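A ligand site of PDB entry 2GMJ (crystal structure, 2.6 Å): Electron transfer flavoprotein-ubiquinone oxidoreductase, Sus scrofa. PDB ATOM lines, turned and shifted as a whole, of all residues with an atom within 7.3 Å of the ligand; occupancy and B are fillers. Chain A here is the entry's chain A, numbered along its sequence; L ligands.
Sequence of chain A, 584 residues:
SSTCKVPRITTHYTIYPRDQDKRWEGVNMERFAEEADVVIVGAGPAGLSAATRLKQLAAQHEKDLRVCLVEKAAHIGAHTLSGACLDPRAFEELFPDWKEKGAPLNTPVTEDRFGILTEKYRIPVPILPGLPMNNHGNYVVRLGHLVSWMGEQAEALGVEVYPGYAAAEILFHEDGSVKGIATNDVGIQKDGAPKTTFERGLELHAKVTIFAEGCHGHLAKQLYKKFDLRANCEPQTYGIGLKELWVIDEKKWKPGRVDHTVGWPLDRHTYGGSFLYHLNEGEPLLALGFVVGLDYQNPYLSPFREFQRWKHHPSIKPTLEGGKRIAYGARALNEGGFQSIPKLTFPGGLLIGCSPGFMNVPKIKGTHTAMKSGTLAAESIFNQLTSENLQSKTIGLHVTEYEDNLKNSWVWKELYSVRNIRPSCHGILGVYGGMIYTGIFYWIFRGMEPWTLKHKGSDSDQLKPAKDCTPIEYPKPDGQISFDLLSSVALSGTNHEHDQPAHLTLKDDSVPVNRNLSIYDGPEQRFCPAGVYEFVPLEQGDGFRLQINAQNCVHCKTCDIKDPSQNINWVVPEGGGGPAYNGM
SG of Cys 528 lies close to N of Ala 530 (3.0 Å). The backbone NH (N) of Trp 570 lies within hydrogen-bond range of the side-chain carboxylate (OD2) of Asp 560 (2.7 Å). The backbone carbonyl oxygen (O) of Val 532 sits at hydrogen-bond distance from the backbone NH (N) of Asn 549 (3.0 Å). The side-chain sulfur of Cys 553 sits close to a ring nitrogen (NE2) of His 503 (3.2 Å). OG1 of Thr 558 sits close to SG of Cys 556, at 2.9 Å. The side-chain sulfur (SG) of Cys 528 sits close to the backbone NH (N) of Val 532 (3.7 Å). SG of Cys 528 lies close to N of Gly 531, at 3.5 Å. The side-chain sulfur (SG) of Cys 559 sits close to the side-chain hydroxyl (OH) of Tyr 533.
Leu 504 touches the ligand (CD1 to S4, 3.4 Å). Pro 529 touches the ligand (CD to S3, 3.6 Å). Val 532 touches the ligand (CB to S4, 3.9 Å). Tyr 533 touches the ligand. Thr 558 touches the ligand. Trp 570 touches the ligand. Hydrophobic or aromatic side chains within 4 Å of the ligand: Leu 504, Pro 529, Val 532, Tyr 533, Val 554 and Trp 570. Within 4 Å of the ligand: Leu 504, Cys 528, Pro 529, Val 532, Tyr 533, Cys 553, Val 554, Cys 556, Lys 557, Thr 558, Cys 559 and Trp 570. The nearest printed residue that does not touch the ligand is His 555 (4.1 Å).
N of Cys 556 sits close to S2 of the ligand. The side-chain sulfur (SG) of Cys 528 is bound to an iron atom (FE2) of the ligand (2.5 Å). A sulfur (S2) of the ligand sits close to the backbone NH (N) of Lys 557. N of Cys 559 sits close to S3 of the ligand (3.6 Å). The backbone NH of Val 554 sits close to a sulfur (S1) of the ligand (3.4 Å). An iron atom (FE1) of the ligand is bound by the side-chain sulfur (SG) of Cys 559 (2.7 Å). SG of Cys 553 is bound to FE3 of the ligand, at 2.5 Å. An iron atom (FE4) of the ligand is bound by the side-chain sulfur (SG) of Cys 556.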
ATOM      1  N   ILE A 240     -30.557   8.644  -5.764  1.00  0.00           N
ATOM      2  CA  ILE A 240     -30.659  10.068  -5.999  1.00  0.00           C
ATOM      3  C   ILE A 240     -31.846  10.594  -5.206  1.00  0.00           C
ATOM      4  O   ILE A 240     -32.948  10.076  -5.309  1.00  0.00           O
ATOM      5  CB  ILE A 240     -30.798  10.421  -7.498  1.00  0.00           C
ATOM      6  CG1 ILE A 240     -30.738  11.946  -7.655  1.00  0.00           C
ATOM      7  CG2 ILE A 240     -32.112   9.888  -8.053  1.00  0.00           C
ATOM      8  CD1 ILE A 240     -31.140  12.427  -9.009  1.00  0.00           C
ATOM      9  N   ALA A 330     -31.701  18.679  -5.207  1.00  0.00           N
ATOM     10  CA  ALA A 330     -31.410  17.259  -5.331  1.00  0.00           C
ATOM     11  C   ALA A 330     -29.969  16.963  -4.952  1.00  0.00           C
ATOM     12  O   ALA A 330     -29.088  17.798  -5.148  1.00  0.00           O
ATOM     13  CB  ALA A 330     -31.680  16.790  -6.752  1.00  0.00           C
ATOM     14  N   HIS A 503     -18.276  22.435 -16.216  1.00  0.00           N
ATOM     15  CA  HIS A 503     -17.650  21.572 -15.224  1.00  0.00           C
ATOM     16  C   HIS A 503     -18.076  20.129 -15.367  1.00  0.00           C
ATOM     17  O   HIS A 503     -17.561  19.252 -14.669  1.00  0.00           O
ATOM     18  CB  HIS A 503     -17.933  22.074 -13.808  1.00  0.00           C
ATOM     19  CG  HIS A 503     -19.382  22.284 -13.527  1.00  0.00           C
ATOM     20  ND1 HIS A 503     -20.115  23.269 -14.140  1.00  0.00           N
ATOM     21  CD2 HIS A 503     -20.230  21.635 -12.700  1.00  0.00           C
ATOM     22  CE1 HIS A 503     -21.367  23.211 -13.718  1.00  0.00           C
ATOM     23  NE2 HIS A 503     -21.460  22.224 -12.838  1.00  0.00           N
ATOM     24  N   LEU A 504     -19.018  19.855 -16.255  1.00  0.00           N
ATOM     25  CA  LEU A 504     -19.418  18.486 -16.495  1.00  0.00           C
ATOM     26  C   LEU A 504     -18.493  18.094 -17.651  1.00  0.00           C
ATOM     27  O   LEU A 504     -18.790  18.360 -18.802  1.00  0.00           O
ATOM     28  CB  LEU A 504     -20.884  18.418 -16.941  1.00  0.00           C
ATOM     29  CG  LEU A 504     -21.956  18.746 -15.892  1.00  0.00           C
ATOM     30  CD1 LEU A 504     -21.822  17.810 -14.698  1.00  0.00           C
ATOM     31  CD2 LEU A 504     -21.808  20.180 -15.426  1.00  0.00           C
ATOM     32  N   GLU A 524     -28.896  10.671 -20.031  1.00  0.00           N
ATOM     33  CA  GLU A 524     -28.484  11.855 -19.326  1.00  0.00           C
ATOM     34  C   GLU A 524     -29.563  12.914 -19.438  1.00  0.00           C
ATOM     35  O   GLU A 524     -29.596  13.854 -18.643  1.00  0.00           O
ATOM     36  CB  GLU A 524     -27.175  12.397 -19.863  1.00  0.00           C
ATOM     37  CG  GLU A 524     -27.119  12.502 -21.363  1.00  0.00           C
ATOM     38  CD  GLU A 524     -26.529  11.254 -22.024  1.00  0.00           C
ATOM     39  OE1 GLU A 524     -25.299  11.246 -22.285  1.00  0.00           O
ATOM     40  OE2 GLU A 524     -27.288  10.297 -22.272  1.00  0.00           O
ATOM     41  N   PHE A 527     -31.868  11.327 -16.278  1.00  0.00           N
ATOM     42  CA  PHE A 527     -31.481  11.083 -14.894  1.00  0.00           C
ATOM     43  C   PHE A 527     -31.000  12.360 -14.218  1.00  0.00           C
ATOM     44  O   PHE A 527     -30.889  12.415 -13.004  1.00  0.00           O
ATOM     45  CB  PHE A 527     -30.458   9.931 -14.745  1.00  0.00           C
ATOM     46  CG  PHE A 527     -29.148  10.151 -15.453  1.00  0.00           C
ATOM     47  CD1 PHE A 527     -28.383  11.283 -15.203  1.00  0.00           C
ATOM     48  CD2 PHE A 527     -28.627   9.171 -16.286  1.00  0.00           C
ATOM     49  CE1 PHE A 527     -27.122  11.417 -15.788  1.00  0.00           C
ATOM     50  CE2 PHE A 527     -27.376   9.301 -16.870  1.00  0.00           C
ATOM     51  CZ  PHE A 527     -26.618  10.422 -16.624  1.00  0.00           C
ATOM     52  N   CYS A 528     -30.733  13.393 -15.009  1.00  0.00           N
ATOM     53  CA  CYS A 528     -30.323  14.662 -14.411  1.00  0.00           C
ATOM     54  C   CYS A 528     -31.561  15.384 -13.897  1.00  0.00           C
ATOM     55  O   CYS A 528     -32.562  15.521 -14.605  1.00  0.00           O
ATOM     56  CB  CYS A 528     -29.657  15.561 -15.420  1.00  0.00           C
ATOM     57  SG  CYS A 528     -29.552  17.205 -14.784  1.00  0.00           S
ATOM     58  N   PRO A 529     -31.504  15.854 -12.657  1.00  0.00           N
ATOM     59  CA  PRO A 529     -32.681  16.559 -12.125  1.00  0.00           C
ATOM     60  C   PRO A 529     -32.749  18.041 -12.446  1.00  0.00           C
ATOM     61  O   PRO A 529     -33.661  18.715 -11.981  1.00  0.00           O
ATOM     62  CB  PRO A 529     -32.579  16.299 -10.633  1.00  0.00           C
ATOM     63  CG  PRO A 529     -31.098  16.349 -10.430  1.00  0.00           C
ATOM     64  CD  PRO A 529     -30.548  15.542 -11.580  1.00  0.00           C
ATOM     65  N   ALA A 530     -31.806  18.543 -13.232  1.00  0.00           N
ATOM     66  CA  ALA A 530     -31.808  19.967 -13.547  1.00  0.00           C
ATOM     67  C   ALA A 530     -31.819  20.296 -15.041  1.00  0.00           C
ATOM     68  O   ALA A 530     -31.521  21.435 -15.436  1.00  0.00           O
ATOM     69  CB  ALA A 530     -30.620  20.630 -12.876  1.00  0.00           C
ATOM     70  N   GLY A 531     -32.170  19.333 -15.880  1.00  0.00           N
ATOM     71  CA  GLY A 531     -32.201  19.566 -17.315  1.00  0.00           C
ATOM     72  C   GLY A 531     -30.922  20.103 -17.952  1.00  0.00           C
ATOM     73  O   GLY A 531     -31.012  20.878 -18.905  1.00  0.00           O
ATOM     74  N   VAL A 532     -29.763  19.697 -17.472  1.00  0.00           N
ATOM     75  CA  VAL A 532     -28.503  20.165 -18.035  1.00  0.00           C
ATOM     76  C   VAL A 532     -28.197  19.539 -19.386  1.00  0.00           C
ATOM     77  O   VAL A 532     -27.721  20.212 -20.282  1.00  0.00           O
ATOM     78  CB  VAL A 532     -27.298  19.873 -17.087  1.00  0.00           C
ATOM     79  CG1 VAL A 532     -25.977  20.001 -17.839  1.00  0.00           C
ATOM     80  CG2 VAL A 532     -27.285  20.864 -15.956  1.00  0.00           C
ATOM     81  N   TYR A 533     -28.472  18.257 -19.546  1.00  0.00           N
ATOM     82  CA  TYR A 533     -28.163  17.622 -20.807  1.00  0.00           C
ATOM     83  C   TYR A 533     -29.342  17.552 -21.742  1.00  0.00           C
ATOM     84  O   TYR A 533     -30.387  17.068 -21.366  1.00  0.00           O
ATOM     85  CB  TYR A 533     -27.681  16.190 -20.581  1.00  0.00           C
ATOM     86  CG  TYR A 533     -26.435  16.094 -19.739  1.00  0.00           C
ATOM     87  CD1 TYR A 533     -26.493  15.588 -18.442  1.00  0.00           C
ATOM     88  CD2 TYR A 533     -25.219  16.591 -20.199  1.00  0.00           C
ATOM     89  CE1 TYR A 533     -25.380  15.578 -17.626  1.00  0.00           C
ATOM     90  CE2 TYR A 533     -24.098  16.585 -19.385  1.00  0.00           C
ATOM     91  CZ  TYR A 533     -24.192  16.085 -18.096  1.00  0.00           C
ATOM     92  OH  TYR A 533     -23.114  16.113 -17.260  1.00  0.00           O
ATOM     93  N   ILE A 548     -24.710  20.943 -23.440  1.00  0.00           N
ATOM     94  CA  ILE A 548     -24.588  20.947 -21.996  1.00  0.00           C
ATOM     95  C   ILE A 548     -24.771  22.340 -21.445  1.00  0.00           C
ATOM     96  O   ILE A 548     -23.950  23.227 -21.711  1.00  0.00           O
ATOM     97  CB  ILE A 548     -23.204  20.433 -21.543  1.00  0.00           C
ATOM     98  CG1 ILE A 548     -22.997  18.983 -21.979  1.00  0.00           C
ATOM     99  CG2 ILE A 548     -23.101  20.532 -20.026  1.00  0.00           C
ATOM    100  CD1 ILE A 548     -21.679  18.387 -21.527  1.00  0.00           C
ATOM    101  N   ASN A 549     -25.853  22.510 -20.685  1.00  0.00           N
ATOM    102  CA  ASN A 549     -26.160  23.799 -20.058  1.00  0.00           C
ATOM    103  C   ASN A 549     -25.574  23.708 -18.674  1.00  0.00           C
ATOM    104  O   ASN A 549     -26.283  23.425 -17.709  1.00  0.00           O
ATOM    105  CB  ASN A 549     -27.664  23.966 -19.963  1.00  0.00           C
ATOM    106  CG  ASN A 549     -28.344  23.817 -21.296  1.00  0.00           C
ATOM    107  OD1 ASN A 549     -27.986  24.495 -22.259  1.00  0.00           O
ATOM    108  ND2 ASN A 549     -29.315  22.922 -21.369  1.00  0.00           N
ATOM    109  N   ALA A 550     -24.280  23.933 -18.562  1.00  0.00           N
ATOM    110  CA  ALA A 550     -23.627  23.784 -17.282  1.00  0.00           C
ATOM    111  C   ALA A 550     -24.153  24.700 -16.209  1.00  0.00           C
ATOM    112  O   ALA A 550     -24.053  24.365 -15.033  1.00  0.00           O
ATOM    113  CB  ALA A 550     -22.128  23.969 -17.438  1.00  0.00           C
ATOM    114  N   ASN A 552     -27.087  25.345 -15.127  1.00  0.00           N
ATOM    115  CA  ASN A 552     -28.176  24.805 -14.338  1.00  0.00           C
ATOM    116  C   ASN A 552     -27.815  23.682 -13.348  1.00  0.00           C
ATOM    117  O   ASN A 552     -28.646  23.227 -12.559  1.00  0.00           O
ATOM    118  CB  ASN A 552     -29.268  24.322 -15.284  1.00  0.00           C
ATOM    119  CG  ASN A 552     -29.869  25.446 -16.076  1.00  0.00           C
ATOM    120  OD1 ASN A 552     -30.472  25.230 -17.125  1.00  0.00           O
ATOM    121  ND2 ASN A 552     -29.723  26.656 -15.556  1.00  0.00           N
ATOM    122  N   CYS A 553     -26.571  23.226 -13.402  1.00  0.00           N
ATOM    123  CA  CYS A 553     -26.131  22.144 -12.546  1.00  0.00           C
ATOM    124  C   CYS A 553     -26.307  22.448 -11.062  1.00  0.00           C
ATOM    125  O   CYS A 553     -25.851  23.485 -10.598  1.00  0.00           O
ATOM    126  CB  CYS A 553     -24.657  21.842 -12.827  1.00  0.00           C
ATOM    127  SG  CYS A 553     -23.930  20.506 -11.826  1.00  0.00           S
ATOM    128  N   VAL A 554     -26.974  21.562 -10.332  1.00  0.00           N
ATOM    129  CA  VAL A 554     -27.177  21.755  -8.901  1.00  0.00           C
ATOM    130  C   VAL A 554     -26.206  20.902  -8.089  1.00  0.00           C
ATOM    131  O   VAL A 554     -26.451  20.614  -6.929  1.00  0.00           O
ATOM    132  CB  VAL A 554     -28.619  21.422  -8.442  1.00  0.00           C
ATOM    133  CG1 VAL A 554     -29.588  22.257  -9.206  1.00  0.00           C
ATOM    134  CG2 VAL A 554     -28.910  19.964  -8.589  1.00  0.00           C
ATOM    135  N   HIS A 555     -25.116  20.495  -8.734  1.00  0.00           N
ATOM    136  CA  HIS A 555     -24.074  19.693  -8.094  1.00  0.00           C
ATOM    137  C   HIS A 555     -24.516  18.434  -7.350  1.00  0.00           C
ATOM    138  O   HIS A 555     -23.949  18.143  -6.290  1.00  0.00           O
ATOM    139  CB  HIS A 555     -23.298  20.550  -7.096  1.00  0.00           C
ATOM    140  CG  HIS A 555     -22.781  21.827  -7.663  1.00  0.00           C
ATOM    141  ND1 HIS A 555     -21.777  22.553  -7.064  1.00  0.00           N
ATOM    142  CD2 HIS A 555     -23.146  22.523  -8.762  1.00  0.00           C
ATOM    143  CE1 HIS A 555     -21.546  23.645  -7.774  1.00  0.00           C
ATOM    144  NE2 HIS A 555     -22.355  23.652  -8.809  1.00  0.00           N
ATOM    145  N   CYS A 556     -25.486  17.675  -7.847  1.00  0.00           N
ATOM    146  CA  CYS A 556     -25.894  16.495  -7.093  1.00  0.00           C
ATOM    147  C   CYS A 556     -24.968  15.302  -7.319  1.00  0.00           C
ATOM    148  O   CYS A 556     -24.928  14.370  -6.510  1.00  0.00           O
ATOM    149  CB  CYS A 556     -27.334  16.117  -7.437  1.00  0.00           C
ATOM    150  SG  CYS A 556     -27.555  15.313  -9.040  1.00  0.00           S
ATOM    151  N   LYS A 557     -24.238  15.356  -8.434  1.00  0.00           N
ATOM    152  CA  LYS A 557     -23.250  14.342  -8.841  1.00  0.00           C
ATOM    153  C   LYS A 557     -23.826  13.093  -9.493  1.00  0.00           C
ATOM    154  O   LYS A 557     -23.082  12.203  -9.906  1.00  0.00           O
ATOM    155  CB  LYS A 557     -22.391  13.925  -7.636  1.00  0.00           C
ATOM    156  CG  LYS A 557     -21.876  15.078  -6.779  1.00  0.00           C
ATOM    157  CD  LYS A 557     -21.115  16.084  -7.603  1.00  0.00           C
ATOM    158  CE  LYS A 557     -20.321  17.029  -6.728  1.00  0.00           C
ATOM    159  NZ  LYS A 557     -19.153  16.394  -6.106  1.00  0.00           N
ATOM    160  N   THR A 558     -25.148  13.018  -9.619  1.00  0.00           N
ATOM    161  CA  THR A 558     -25.790  11.843 -10.209  1.00  0.00           C
ATOM    162  C   THR A 558     -25.295  11.414 -11.593  1.00  0.00           C
ATOM    163  O   THR A 558     -25.239  10.213 -11.898  1.00  0.00           O
ATOM    164  CB  THR A 558     -27.322  12.035 -10.294  1.00  0.00           C
ATOM    165  OG1 THR A 558     -27.821  12.446  -9.014  1.00  0.00           O
ATOM    166  CG2 THR A 558     -28.031  10.746 -10.711  1.00  0.00           C
ATOM    167  N   CYS A 559     -24.916  12.374 -12.426  1.00  0.00           N
ATOM    168  CA  CYS A 559     -24.483  12.029 -13.778  1.00  0.00           C
ATOM    169  C   CYS A 559     -23.141  11.308 -13.799  1.00  0.00           C
ATOM    170  O   CYS A 559     -22.927  10.422 -14.623  1.00  0.00           O
ATOM    171  CB  CYS A 559     -24.409  13.286 -14.643  1.00  0.00           C
ATOM    172  SG  CYS A 559     -22.982  14.341 -14.234  1.00  0.00           S
ATOM    173  N   ASP A 560     -22.235  11.702 -12.903  1.00  0.00           N
ATOM    174  CA  ASP A 560     -20.906  11.095 -12.820  1.00  0.00           C
ATOM    175  C   ASP A 560     -21.080   9.656 -12.384  1.00  0.00           C
ATOM    176  O   ASP A 560     -20.267   8.781 -12.691  1.00  0.00           O
ATOM    177  CB  ASP A 560     -20.057  11.832 -11.794  1.00  0.00           C
ATOM    178  CG  ASP A 560     -18.609  11.457 -11.868  1.00  0.00           C
ATOM    179  OD1 ASP A 560     -18.314  10.248 -11.766  1.00  0.00           O
ATOM    180  OD2 ASP A 560     -17.769  12.374 -12.040  1.00  0.00           O
ATOM    181  N   ILE A 561     -22.163   9.407 -11.671  1.00  0.00           N
ATOM    182  CA  ILE A 561     -22.429   8.077 -11.180  1.00  0.00           C
ATOM    183  C   ILE A 561     -23.145   7.176 -12.176  1.00  0.00           C
ATOM    184  O   ILE A 561     -22.647   6.109 -12.501  1.00  0.00           O
ATOM    185  CB  ILE A 561     -23.261   8.138  -9.859  1.00  0.00           C
ATOM    186  CG1 ILE A 561     -22.425   8.814  -8.768  1.00  0.00           C
ATOM    187  CG2 ILE A 561     -23.641   6.759  -9.407  1.00  0.00           C
ATOM    188  CD1 ILE A 561     -23.208   9.141  -7.539  1.00  0.00           C
ATOM    189  N   ILE A 568     -18.485  10.750 -18.248  1.00  0.00           N
ATOM    190  CA  ILE A 568     -18.594  12.020 -17.552  1.00  0.00           C
ATOM    191  C   ILE A 568     -17.779  12.091 -16.260  1.00  0.00           C
ATOM    192  O   ILE A 568     -17.731  11.125 -15.508  1.00  0.00           O
ATOM    193  CB  ILE A 568     -20.072  12.300 -17.187  1.00  0.00           C
ATOM    194  CG1 ILE A 568     -20.917  12.364 -18.453  1.00  0.00           C
ATOM    195  CG2 ILE A 568     -20.208  13.585 -16.378  1.00  0.00           C
ATOM    196  CD1 ILE A 568     -22.390  12.448 -18.165  1.00  0.00           C
ATOM    197  N   TRP A 570     -17.617  14.799 -13.115  1.00  0.00           N
ATOM    198  CA  TRP A 570     -17.987  16.036 -12.460  1.00  0.00           C
ATOM    199  C   TRP A 570     -16.800  16.698 -11.789  1.00  0.00           C
ATOM    200  O   TRP A 570     -16.094  16.076 -10.986  1.00  0.00           O
ATOM    201  CB  TRP A 570     -19.066  15.779 -11.418  1.00  0.00           C
ATOM    202  CG  TRP A 570     -19.727  17.046 -10.950  1.00  0.00           C
ATOM    203  CD1 TRP A 570     -20.905  17.558 -11.412  1.00  0.00           C
ATOM    204  CD2 TRP A 570     -19.246  17.965  -9.964  1.00  0.00           C
ATOM    205  NE1 TRP A 570     -21.188  18.734 -10.772  1.00  0.00           N
ATOM    206  CE2 TRP A 570     -20.181  19.012  -9.878  1.00  0.00           C
ATOM    207  CE3 TRP A 570     -18.107  17.998  -9.145  1.00  0.00           C
ATOM    208  CZ2 TRP A 570     -20.017  20.097  -9.017  1.00  0.00           C
ATOM    209  CZ3 TRP A 570     -17.943  19.084  -8.284  1.00  0.00           C
ATOM    210  CH2 TRP A 570     -18.897  20.117  -8.223  1.00  0.00           C
HETATM  211 FE1  LIG L   1     -25.004  15.836 -13.301  1.00  0.00          FE
HETATM  212 FE2  LIG L   1     -27.313  17.253 -13.598  1.00  0.00          FE
HETATM  213 FE3  LIG L   1     -25.097  18.412 -12.347  1.00  0.00          FE
HETATM  214 FE4  LIG L   1     -26.498  16.429 -10.997  1.00  0.00          FE
HETATM  215  S1  LIG L   1     -27.222  18.436 -11.582  1.00  0.00           S
HETATM  216  S2  LIG L   1     -24.323  16.604 -11.235  1.00  0.00           S
HETATM  217  S3  LIG L   1     -27.119  15.186 -12.719  1.00  0.00           S
HETATM  218  S4  LIG L   1     -25.252  17.778 -14.449  1.00  0.00           S
